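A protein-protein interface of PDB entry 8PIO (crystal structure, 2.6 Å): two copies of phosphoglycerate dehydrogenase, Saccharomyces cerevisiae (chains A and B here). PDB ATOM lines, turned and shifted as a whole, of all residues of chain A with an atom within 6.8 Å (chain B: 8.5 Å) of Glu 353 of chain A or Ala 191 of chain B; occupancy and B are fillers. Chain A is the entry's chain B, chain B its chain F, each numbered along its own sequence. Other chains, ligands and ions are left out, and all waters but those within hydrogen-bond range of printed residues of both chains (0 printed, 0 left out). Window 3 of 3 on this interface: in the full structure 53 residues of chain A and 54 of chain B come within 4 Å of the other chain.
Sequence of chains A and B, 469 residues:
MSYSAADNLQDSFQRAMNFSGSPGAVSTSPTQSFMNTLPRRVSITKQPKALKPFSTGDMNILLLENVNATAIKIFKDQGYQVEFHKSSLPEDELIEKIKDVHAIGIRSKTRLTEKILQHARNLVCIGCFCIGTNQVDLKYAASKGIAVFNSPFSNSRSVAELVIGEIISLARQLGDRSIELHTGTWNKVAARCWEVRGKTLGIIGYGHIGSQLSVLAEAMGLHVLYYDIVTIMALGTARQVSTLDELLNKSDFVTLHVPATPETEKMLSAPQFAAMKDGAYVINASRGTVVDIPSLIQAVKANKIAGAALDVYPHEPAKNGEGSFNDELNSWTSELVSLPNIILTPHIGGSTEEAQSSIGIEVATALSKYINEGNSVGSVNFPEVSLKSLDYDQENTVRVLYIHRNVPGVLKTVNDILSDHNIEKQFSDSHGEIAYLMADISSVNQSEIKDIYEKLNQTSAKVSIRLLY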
ATOM      1  N   ASN A  68      -8.685   3.753  -6.655  1.00  0.00           N
ATOM      2  CA  ASN A  68      -8.039   3.613  -7.984  1.00  0.00           C
ATOM      3  C   ASN A  68      -8.144   2.156  -8.464  1.00  0.00           C
ATOM      4  O   ASN A  68      -8.228   1.266  -7.613  1.00  0.00           O
ATOM      5  CB  ASN A  68      -6.590   4.088  -7.940  1.00  0.00           C
ATOM      6  CG  ASN A  68      -6.006   4.286  -9.315  1.00  0.00           C
ATOM      7  OD1 ASN A  68      -5.820   3.320 -10.062  1.00  0.00           O
ATOM      8  ND2 ASN A  68      -5.714   5.532  -9.657  1.00  0.00           N
ATOM      9  N   SER A 158       3.383  15.219  -6.416  1.00  0.00           N
ATOM     10  CA  SER A 158       2.214  15.972  -6.945  1.00  0.00           C
ATOM     11  C   SER A 158       2.176  17.382  -6.352  1.00  0.00           C
ATOM     12  O   SER A 158       1.855  18.326  -7.099  1.00  0.00           O
ATOM     13  CB  SER A 158       0.940  15.234  -6.698  1.00  0.00           C
ATOM     14  OG  SER A 158       0.851  14.087  -7.546  1.00  0.00           O
ATOM     15  N   GLY A 350      -2.468  16.877  -4.043  1.00  0.00           N
ATOM     16  CA  GLY A 350      -2.252  15.444  -4.334  1.00  0.00           C
ATOM     17  C   GLY A 350      -3.296  14.884  -5.279  1.00  0.00           C
ATOM     18  O   GLY A 350      -3.398  13.640  -5.378  1.00  0.00           O
ATOM     19  N   SER A 351      -4.028  15.758  -5.964  1.00  0.00           N
ATOM     20  CA  SER A 351      -5.145  15.400  -6.874  1.00  0.00           C
ATOM     21  C   SER A 351      -4.606  15.094  -8.272  1.00  0.00           C
ATOM     22  O   SER A 351      -4.783  15.955  -9.173  1.00  0.00           O
ATOM     23  CB  SER A 351      -6.182  16.496  -6.901  1.00  0.00           C
ATOM     24  OG  SER A 351      -6.813  16.621  -5.629  1.00  0.00           O
ATOM     25  N   THR A 352      -3.971  13.924  -8.444  1.00  0.00           N
ATOM     26  CA  THR A 352      -3.425  13.434  -9.750  1.00  0.00           C
ATOM     27  C   THR A 352      -3.659  11.927  -9.893  1.00  0.00           C
ATOM     28  O   THR A 352      -3.751  11.250  -8.874  1.00  0.00           O
ATOM     29  CB  THR A 352      -1.931  13.743  -9.902  1.00  0.00           C
ATOM     30  OG1 THR A 352      -1.207  12.933  -8.977  1.00  0.00           O
ATOM     31  CG2 THR A 352      -1.609  15.205  -9.686  1.00  0.00           C
ATOM     32  N   GLU A 353      -3.737  11.445 -11.133  1.00  0.00           N
ATOM     33  CA  GLU A 353      -3.933  10.012 -11.466  1.00  0.00           C
ATOM     34  C   GLU A 353      -2.746   9.212 -10.925  1.00  0.00           C
ATOM     35  O   GLU A 353      -2.962   8.108 -10.437  1.00  0.00           O
ATOM     36  CB  GLU A 353      -4.077   9.830 -12.976  1.00  0.00           C
ATOM     37  CG  GLU A 353      -5.336  10.455 -13.545  1.00  0.00           C
ATOM     38  CD  GLU A 353      -6.566   9.561 -13.513  1.00  0.00           C
ATOM     39  OE1 GLU A 353      -6.543   8.548 -12.793  1.00  0.00           O
ATOM     40  OE2 GLU A 353      -7.547   9.880 -14.226  1.00  0.00           O
ATOM     41  N   GLU A 354      -1.537   9.769 -11.021  1.00  0.00           N
ATOM     42  CA  GLU A 354      -0.289   9.155 -10.484  1.00  0.00           C
ATOM     43  C   GLU A 354      -0.471   8.875  -8.994  1.00  0.00           C
ATOM     44  O   GLU A 354      -0.364   7.711  -8.606  1.00  0.00           O
ATOM     45  CB  GLU A 354       0.913  10.076 -10.722  1.00  0.00           C
ATOM     46  CG  GLU A 354       1.461  10.003 -12.130  1.00  0.00           C
ATOM     47  CD  GLU A 354       0.495  10.458 -13.210  1.00  0.00           C
ATOM     48  OE1 GLU A 354      -0.163  11.521 -13.012  1.00  0.00           O
ATOM     49  OE2 GLU A 354       0.385   9.746 -14.249  1.00  0.00           O
ATOM     50  N   ALA A 355      -0.734   9.920  -8.210  1.00  0.00           N
ATOM     51  CA  ALA A 355      -0.905   9.875  -6.739  1.00  0.00           C
ATOM     52  C   ALA A 355      -1.917   8.782  -6.356  1.00  0.00           C
ATOM     53  O   ALA A 355      -1.557   7.894  -5.564  1.00  0.00           O
ATOM     54  CB  ALA A 355      -1.341  11.227  -6.235  1.00  0.00           C
ATOM     55  N   GLN A 356      -3.128   8.854  -6.901  1.00  0.00           N
ATOM     56  CA  GLN A 356      -4.242   7.899  -6.615  1.00  0.00           C
ATOM     57  C   GLN A 356      -3.812   6.482  -7.000  1.00  0.00           C
ATOM     58  O   GLN A 356      -4.139   5.553  -6.263  1.00  0.00           O
ATOM     59  CB  GLN A 356      -5.513   8.301  -7.365  1.00  0.00           C
ATOM     60  CG  GLN A 356      -6.138   9.585  -6.844  1.00  0.00           C
ATOM     61  CD  GLN A 356      -6.359   9.537  -5.351  1.00  0.00           C
ATOM     62  OE1 GLN A 356      -7.200   8.796  -4.855  1.00  0.00           O
ATOM     63  NE2 GLN A 356      -5.580  10.329  -4.621  1.00  0.00           N
ATOM     64  N   SER A 357      -3.103   6.345  -8.111  1.00  0.00           N
ATOM     65  CA  SER A 357      -2.595   5.055  -8.648  1.00  0.00           C
ATOM     66  C   SER A 357      -1.648   4.406  -7.624  1.00  0.00           C
ATOM     67  O   SER A 357      -1.888   3.228  -7.248  1.00  0.00           O
ATOM     68  CB  SER A 357      -1.924   5.253  -9.990  1.00  0.00           C
ATOM     69  OG  SER A 357      -1.355   4.042 -10.465  1.00  0.00           O
ATOM     70  N   SER A 358      -0.626   5.140  -7.185  1.00  0.00           N
ATOM     71  CA  SER A 358       0.413   4.652  -6.236  1.00  0.00           C
ATOM     72  C   SER A 358      -0.200   4.453  -4.838  1.00  0.00           C
ATOM     73  O   SER A 358       0.263   3.549  -4.127  1.00  0.00           O
ATOM     74  CB  SER A 358       1.629   5.567  -6.206  1.00  0.00           C
ATOM     75  OG  SER A 358       1.250   6.928  -6.177  1.00  0.00           O
ATOM     76  N   LEU B 170      -1.678  23.090 -17.282  1.00  0.00           N
ATOM     77  CA  LEU B 170      -2.626  22.308 -18.120  1.00  0.00           C
ATOM     78  C   LEU B 170      -2.788  20.907 -17.534  1.00  0.00           C
ATOM     79  O   LEU B 170      -3.926  20.418 -17.460  1.00  0.00           O
ATOM     80  CB  LEU B 170      -2.086  22.232 -19.550  1.00  0.00           C
ATOM     81  CG  LEU B 170      -2.108  23.533 -20.339  1.00  0.00           C
ATOM     82  CD1 LEU B 170      -1.388  23.358 -21.668  1.00  0.00           C
ATOM     83  CD2 LEU B 170      -3.536  24.013 -20.557  1.00  0.00           C
ATOM     84  N   ALA B 171      -1.678  20.290 -17.156  1.00  0.00           N
ATOM     85  CA  ALA B 171      -1.604  18.935 -16.564  1.00  0.00           C
ATOM     86  C   ALA B 171      -2.531  18.840 -15.343  1.00  0.00           C
ATOM     87  O   ALA B 171      -3.070  17.747 -15.098  1.00  0.00           O
ATOM     88  CB  ALA B 171      -0.180  18.621 -16.188  1.00  0.00           C
ATOM     89  N   ARG B 172      -2.697  19.946 -14.612  1.00  0.00           N
ATOM     90  CA  ARG B 172      -3.411  19.992 -13.304  1.00  0.00           C
ATOM     91  C   ARG B 172      -4.686  20.839 -13.414  1.00  0.00           C
ATOM     92  O   ARG B 172      -5.487  20.805 -12.473  1.00  0.00           O
ATOM     93  CB  ARG B 172      -2.482  20.552 -12.228  1.00  0.00           C
ATOM     94  CG  ARG B 172      -1.197  19.754 -12.047  1.00  0.00           C
ATOM     95  CD  ARG B 172      -1.426  18.379 -11.452  1.00  0.00           C
ATOM     96  NE  ARG B 172      -1.736  18.437 -10.035  1.00  0.00           N
ATOM     97  CZ  ARG B 172      -0.831  18.554  -9.063  1.00  0.00           C
ATOM     98  NH1 ARG B 172       0.457  18.628  -9.355  1.00  0.00           N
ATOM     99  NH2 ARG B 172      -1.222  18.600  -7.804  1.00  0.00           N
ATOM    100  N   GLN B 173      -4.851  21.562 -14.523  1.00  0.00           N
ATOM    101  CA  GLN B 173      -6.011  22.460 -14.785  1.00  0.00           C
ATOM    102  C   GLN B 173      -6.057  23.563 -13.716  1.00  0.00           C
ATOM    103  O   GLN B 173      -7.133  23.799 -13.175  1.00  0.00           O
ATOM    104  CB  GLN B 173      -7.326  21.668 -14.795  1.00  0.00           C
ATOM    105  CG  GLN B 173      -7.341  20.509 -15.780  1.00  0.00           C
ATOM    106  CD  GLN B 173      -8.612  19.691 -15.692  1.00  0.00           C
ATOM    107  OE1 GLN B 173      -9.647  20.159 -15.222  1.00  0.00           O
ATOM    108  NE2 GLN B 173      -8.539  18.449 -16.149  1.00  0.00           N
ATOM    109  N   ARG B 177      -9.354  25.589 -11.999  1.00  0.00           N
ATOM    110  CA  ARG B 177      -9.519  25.410 -10.527  1.00  0.00           C
ATOM    111  C   ARG B 177      -9.612  26.778  -9.846  1.00  0.00           C
ATOM    112  O   ARG B 177     -10.520  26.970  -9.029  1.00  0.00           O
ATOM    113  CB  ARG B 177      -8.345  24.625  -9.942  1.00  0.00           C
ATOM    114  CG  ARG B 177      -8.317  23.153 -10.322  1.00  0.00           C
ATOM    115  CD  ARG B 177      -9.562  22.426  -9.879  1.00  0.00           C
ATOM    116  NE  ARG B 177     -10.567  22.443 -10.914  1.00  0.00           N
ATOM    117  CZ  ARG B 177     -10.577  21.633 -11.955  1.00  0.00           C
ATOM    118  NH1 ARG B 177     -11.538  21.734 -12.859  1.00  0.00           N
ATOM    119  NH2 ARG B 177      -9.626  20.719 -12.095  1.00  0.00           N
ATOM    120  N   LYS B 188     -12.708  19.952  -6.479  1.00  0.00           N
ATOM    121  CA  LYS B 188     -11.519  19.084  -6.267  1.00  0.00           C
ATOM    122  C   LYS B 188     -11.603  17.899  -7.236  1.00  0.00           C
ATOM    123  O   LYS B 188     -12.432  17.028  -7.013  1.00  0.00           O
ATOM    124  CB  LYS B 188     -11.450  18.626  -4.810  1.00  0.00           C
ATOM    125  CG  LYS B 188     -10.292  17.695  -4.471  1.00  0.00           C
ATOM    126  CD  LYS B 188     -10.352  17.170  -3.049  1.00  0.00           C
ATOM    127  CE  LYS B 188      -9.066  16.516  -2.588  1.00  0.00           C
ATOM    128  NZ  LYS B 188      -8.853  16.694  -1.127  1.00  0.00           N
ATOM    129  N   VAL B 189     -10.761  17.899  -8.269  1.00  0.00           N
ATOM    130  CA  VAL B 189     -10.774  16.901  -9.381  1.00  0.00           C
ATOM    131  C   VAL B 189      -9.357  16.369  -9.596  1.00  0.00           C
ATOM    132  O   VAL B 189      -8.426  17.193  -9.732  1.00  0.00           O
ATOM    133  CB  VAL B 189     -11.324  17.522 -10.677  1.00  0.00           C
ATOM    134  CG1 VAL B 189     -11.180  16.568 -11.867  1.00  0.00           C
ATOM    135  CG2 VAL B 189     -12.768  17.973 -10.507  1.00  0.00           C
ATOM    136  N   ALA B 190      -9.214  15.044  -9.643  1.00  0.00           N
ATOM    137  CA  ALA B 190      -7.945  14.330  -9.921  1.00  0.00           C
ATOM    138  C   ALA B 190      -8.043  13.584 -11.259  1.00  0.00           C
ATOM    139  O   ALA B 190      -6.997  13.150 -11.765  1.00  0.00           O
ATOM    140  CB  ALA B 190      -7.629  13.385  -8.787  1.00  0.00           C
ATOM    141  N   ALA B 191      -9.252  13.445 -11.799  1.00  0.00           N
ATOM    142  CA  ALA B 191      -9.537  12.730 -13.067  1.00  0.00           C
ATOM    143  C   ALA B 191      -8.808  13.424 -14.217  1.00  0.00           C
ATOM    144  O   ALA B 191      -9.021  14.649 -14.409  1.00  0.00           O
ATOM    145  CB  ALA B 191     -11.020  12.678 -13.318  1.00  0.00           C
ATOM    146  N   ARG B 192      -7.974  12.675 -14.937  1.00  0.00           N
ATOM    147  CA  ARG B 192      -7.200  13.152 -16.108  1.00  0.00           C
ATOM    148  C   ARG B 192      -6.444  14.442 -15.725  1.00  0.00           C
ATOM    149  O   ARG B 192      -6.307  15.338 -16.581  1.00  0.00           O
ATOM    150  CB  ARG B 192      -8.135  13.329 -17.302  1.00  0.00           C
ATOM    151  CG  ARG B 192      -9.031  12.119 -17.558  1.00  0.00           C
ATOM    152  CD  ARG B 192      -9.365  11.875 -19.024  1.00  0.00           C
ATOM    153  NE  ARG B 192      -8.477  10.896 -19.661  1.00  0.00           N
ATOM    154  CZ  ARG B 192      -7.422  11.205 -20.417  1.00  0.00           C
ATOM    155  NH1 ARG B 192      -6.686  10.242 -20.951  1.00  0.00           N
ATOM    156  NH2 ARG B 192      -7.105  12.471 -20.638  1.00  0.00           N
ATOM    157  N   CYS B 193      -5.995  14.518 -14.473  1.00  0.00           N
ATOM    158  CA  CYS B 193      -4.968  15.476 -13.970  1.00  0.00           C
ATOM    159  C   CYS B 193      -3.693  14.690 -13.643  1.00  0.00           C
ATOM    160  O   CYS B 193      -3.808  13.660 -12.961  1.00  0.00           O
ATOM    161  CB  CYS B 193      -5.463  16.230 -12.744  1.00  0.00           C
ATOM    162  SG  CYS B 193      -6.720  17.475 -13.129  1.00  0.00           S
ATOM    163  N   TRP B 194      -2.526  15.153 -14.117  1.00  0.00           N
ATOM    164  CA  TRP B 194      -1.285  14.329 -14.185  1.00  0.00           C
ATOM    165  C   TRP B 194      -0.114  14.992 -13.480  1.00  0.00           C
ATOM    166  O   TRP B 194      -0.014  16.234 -13.511  1.00  0.00           O
ATOM    167  CB  TRP B 194      -0.917  14.038 -15.633  1.00  0.00           C
ATOM    168  CG  TRP B 194      -2.084  13.783 -16.517  1.00  0.00           C
ATOM    169  CD1 TRP B 194      -2.731  14.687 -17.302  1.00  0.00           C
ATOM    170  CD2 TRP B 194      -2.748  12.532 -16.711  1.00  0.00           C
ATOM    171  NE1 TRP B 194      -3.749  14.083 -17.977  1.00  0.00           N
ATOM    172  CE2 TRP B 194      -3.785  12.759 -17.636  1.00  0.00           C
ATOM    173  CE3 TRP B 194      -2.568  11.243 -16.204  1.00  0.00           C
ATOM    174  CZ2 TRP B 194      -4.636  11.744 -18.060  1.00  0.00           C
ATOM    175  CZ3 TRP B 194      -3.410  10.237 -16.625  1.00  0.00           C
ATOM    176  CH2 TRP B 194      -4.429  10.488 -17.540  1.00  0.00           C
ATOM    177  N   GLU B 195       0.746  14.166 -12.886  1.00  0.00           N
ATOM    178  CA  GLU B 195       2.175  14.470 -12.671  1.00  0.00           C
ATOM    179  C   GLU B 195       2.830  14.531 -14.047  1.00  0.00           C
ATOM    180  O   GLU B 195       2.522  13.654 -14.874  1.00  0.00           O
ATOM    181  CB  GLU B 195       2.852  13.389 -11.828  1.00  0.00           C
ATOM    182  CG  GLU B 195       2.334  13.295 -10.414  1.00  0.00           C
ATOM    183  CD  GLU B 195       3.008  12.225  -9.582  1.00  0.00           C
ATOM    184  OE1 GLU B 195       3.835  11.441 -10.160  1.00  0.00           O
ATOM    185  OE2 GLU B 195       2.729  12.167  -8.363  1.00  0.00           O
ATOM    186  N   LYS B 199       5.851  11.621 -18.278  1.00  0.00           N
ATOM    187  CA  LYS B 199       5.133  12.067 -19.506  1.00  0.00           C
ATOM    188  C   LYS B 199       6.157  12.423 -20.583  1.00  0.00           C
ATOM    189  O   LYS B 199       7.338  12.629 -20.237  1.00  0.00           O
ATOM    190  CB  LYS B 199       4.233  13.271 -19.215  1.00  0.00           C
ATOM    191  CG  LYS B 199       3.110  13.016 -18.223  1.00  0.00           C
ATOM    192  CD  LYS B 199       2.117  11.993 -18.688  1.00  0.00           C
ATOM    193  CE  LYS B 199       0.987  11.784 -17.708  1.00  0.00           C
ATOM    194  NZ  LYS B 199       1.491  11.342 -16.388  1.00  0.00           N
ATOM    195  N   TYR B 281      -1.983  17.599 -25.152  1.00  0.00           N
ATOM    196  CA  TYR B 281      -1.965  19.068 -24.886  1.00  0.00           C
ATOM    197  C   TYR B 281      -1.120  19.776 -25.942  1.00  0.00           C
ATOM    198  O   TYR B 281      -0.056  19.255 -26.311  1.00  0.00           O
ATOM    199  CB  TYR B 281      -1.427  19.356 -23.483  1.00  0.00           C
ATOM    200  CG  TYR B 281      -2.176  18.680 -22.360  1.00  0.00           C
ATOM    201  CD1 TYR B 281      -1.844  17.396 -21.945  1.00  0.00           C
ATOM    202  CD2 TYR B 281      -3.213  19.324 -21.701  1.00  0.00           C
ATOM    203  CE1 TYR B 281      -2.530  16.771 -20.914  1.00  0.00           C
ATOM    204  CE2 TYR B 281      -3.907  18.714 -20.668  1.00  0.00           C
ATOM    205  CZ  TYR B 281      -3.567  17.437 -20.273  1.00  0.00           C
ATOM    206  OH  TYR B 281      -4.245  16.837 -19.260  1.00  0.00           O
ATOM    207  N   ALA B 306      -7.011  17.711 -24.461  1.00  0.00           N
ATOM    208  CA  ALA B 306      -7.432  17.908 -23.056  1.00  0.00           C
ATOM    209  C   ALA B 306      -7.211  19.366 -22.636  1.00  0.00           C
ATOM    210  O   ALA B 306      -7.845  19.792 -21.675  1.00  0.00           O
ATOM    211  CB  ALA B 306      -6.684  16.956 -22.162  1.00  0.00           C
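No position is printed for both chains. Of the 18 pairs that touch across the chains among the printed residues, none has its exchanged pair printed and touching as well.
Ser 351 of chain A touches Lys 188 of chain B. Val 189 of chain B touches Ser 351 of chain A. CB of Cys 193 of chain B touches O of Ser 351 of chain A, at 3.6 Å. Arg 172 of chain B touches Thr 352 of chain A. Thr 352 of chain A touches Ala 190 of chain B. Thr 352 of chain A touches Cys 193 of chain B. Thr 352 of chain A touches Glu 195 of chain B. O of Ala 190 of chain B touches CG of Glu 353 of chain A, 3.6 Å away. CG of Glu 353 of chain A touches CZ3 of Trp 194 of chain B, at 3.6 Å. Trp 194 of chain B touches Glu 354 of chain A.
The backbone NH (N) of Trp 194 of chain B is in hydrogen-bond range of the backbone carbonyl oxygen (O) of Ala 171 of chain B, at 2.8 Å. O of Arg 172 of chain B lies within hydrogen-bond range of SG of Cys 193 of chain B, at 3.6 Å. The side-chain amide nitrogen (NE2) of Gln 173 of chain B sits at hydrogen-bond distance from the side-chain sulfur (SG) of Cys 193 of chain B (3.7 Å). The side-chain amino group (NZ) of Lys 199 of chain B is in hydrogen-bond range of the backbone carbonyl oxygen (O) of Glu 195 of chain B (2.9 Å). OG1 of Thr 352 of chain A sits at hydrogen-bond distance from OG of Ser 158 of chain A. O of Glu 354 of chain A lies within hydrogen-bond range of OG of Ser 358 of chain A (3.0 Å).
Of the 11 printed residues of chain A, 5 touch a printed residue of chain B. Printed residues of chain B that touch a printed residue of chain A: Arg 172, Lys 188, Val 189, Ala 190, Ala 191, Arg 192, Cys 193, Trp 194, Glu 195 and Lys 199. Among the printed residues, 18 pairs touch across the chains. Among the printed residues, Asp or Glu carboxylates within 4 Å of a Lys or Arg side-chain nitrogen of the other chain: Glu 354 of chain A with Lys 199 of chain B (2.9 Å).
The guanidinium group (NH1) of Arg 172 of chain B is in hydrogen-bond range of the backbone carbonyl oxygen (O) of Ser 158 of chain A (2.7 Å). The backbone NH of Arg 192 of chain B lies within hydrogen-bond range of the side-chain carboxylate of Glu 353 of chain A (2.9 Å). The backbone carbonyl oxygen (O) of Cys 193 of chain B sits at hydrogen-bond distance from the backbone NH (N) of Glu 353 of chain A (2.9 Å). The side-chain hydroxyl (OG) of Ser 158 of chain A is in hydrogen-bond range of the side-chain carboxylate (OE2) of Glu 195 of chain B, at 2.8 Å. N of Glu 195 of chain B lies within hydrogen-bond range of OE1 of Glu 354 of chain A, 2.8 Å away. NZ of Lys 199 of chain B is in salt-bridge range of OE2 of Glu 354 of chain A.
Of the printed residues of chain B, Thr 352 of chain A touches Arg 172 (3.3 Å), Ala 190 (3.7 Å), Cys 193 (3.2 Å) and Glu 195 (3.8 Å). Glu 353 of chain A touches just these residues of chain B: Ala 190 (3.6 Å), Ala 191 (3.7 Å), Arg 192 (2.9 Å), Cys 193 (2.9 Å) and Trp 194 (3.6 Å). Gln 356 of chain A touches none of the printed residues of chain B. Of chain A, only Glu 353 comes within 4 Å of Ala 191 of chain B. Printed residues of chain A within 4 Å of Cys 193 of chain B: Ser 351 (3.6 Å), Thr 352 (3.2 Å) and Glu 353 (2.9 Å). The nearest residue of chain B that does not touch Glu 353 of chain A is Glu 195 of chain B (5.5 Å). The nearest printed residue of chain B that does not touch Ser 351 of chain A is Arg 172 of chain B (4.02 Å).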
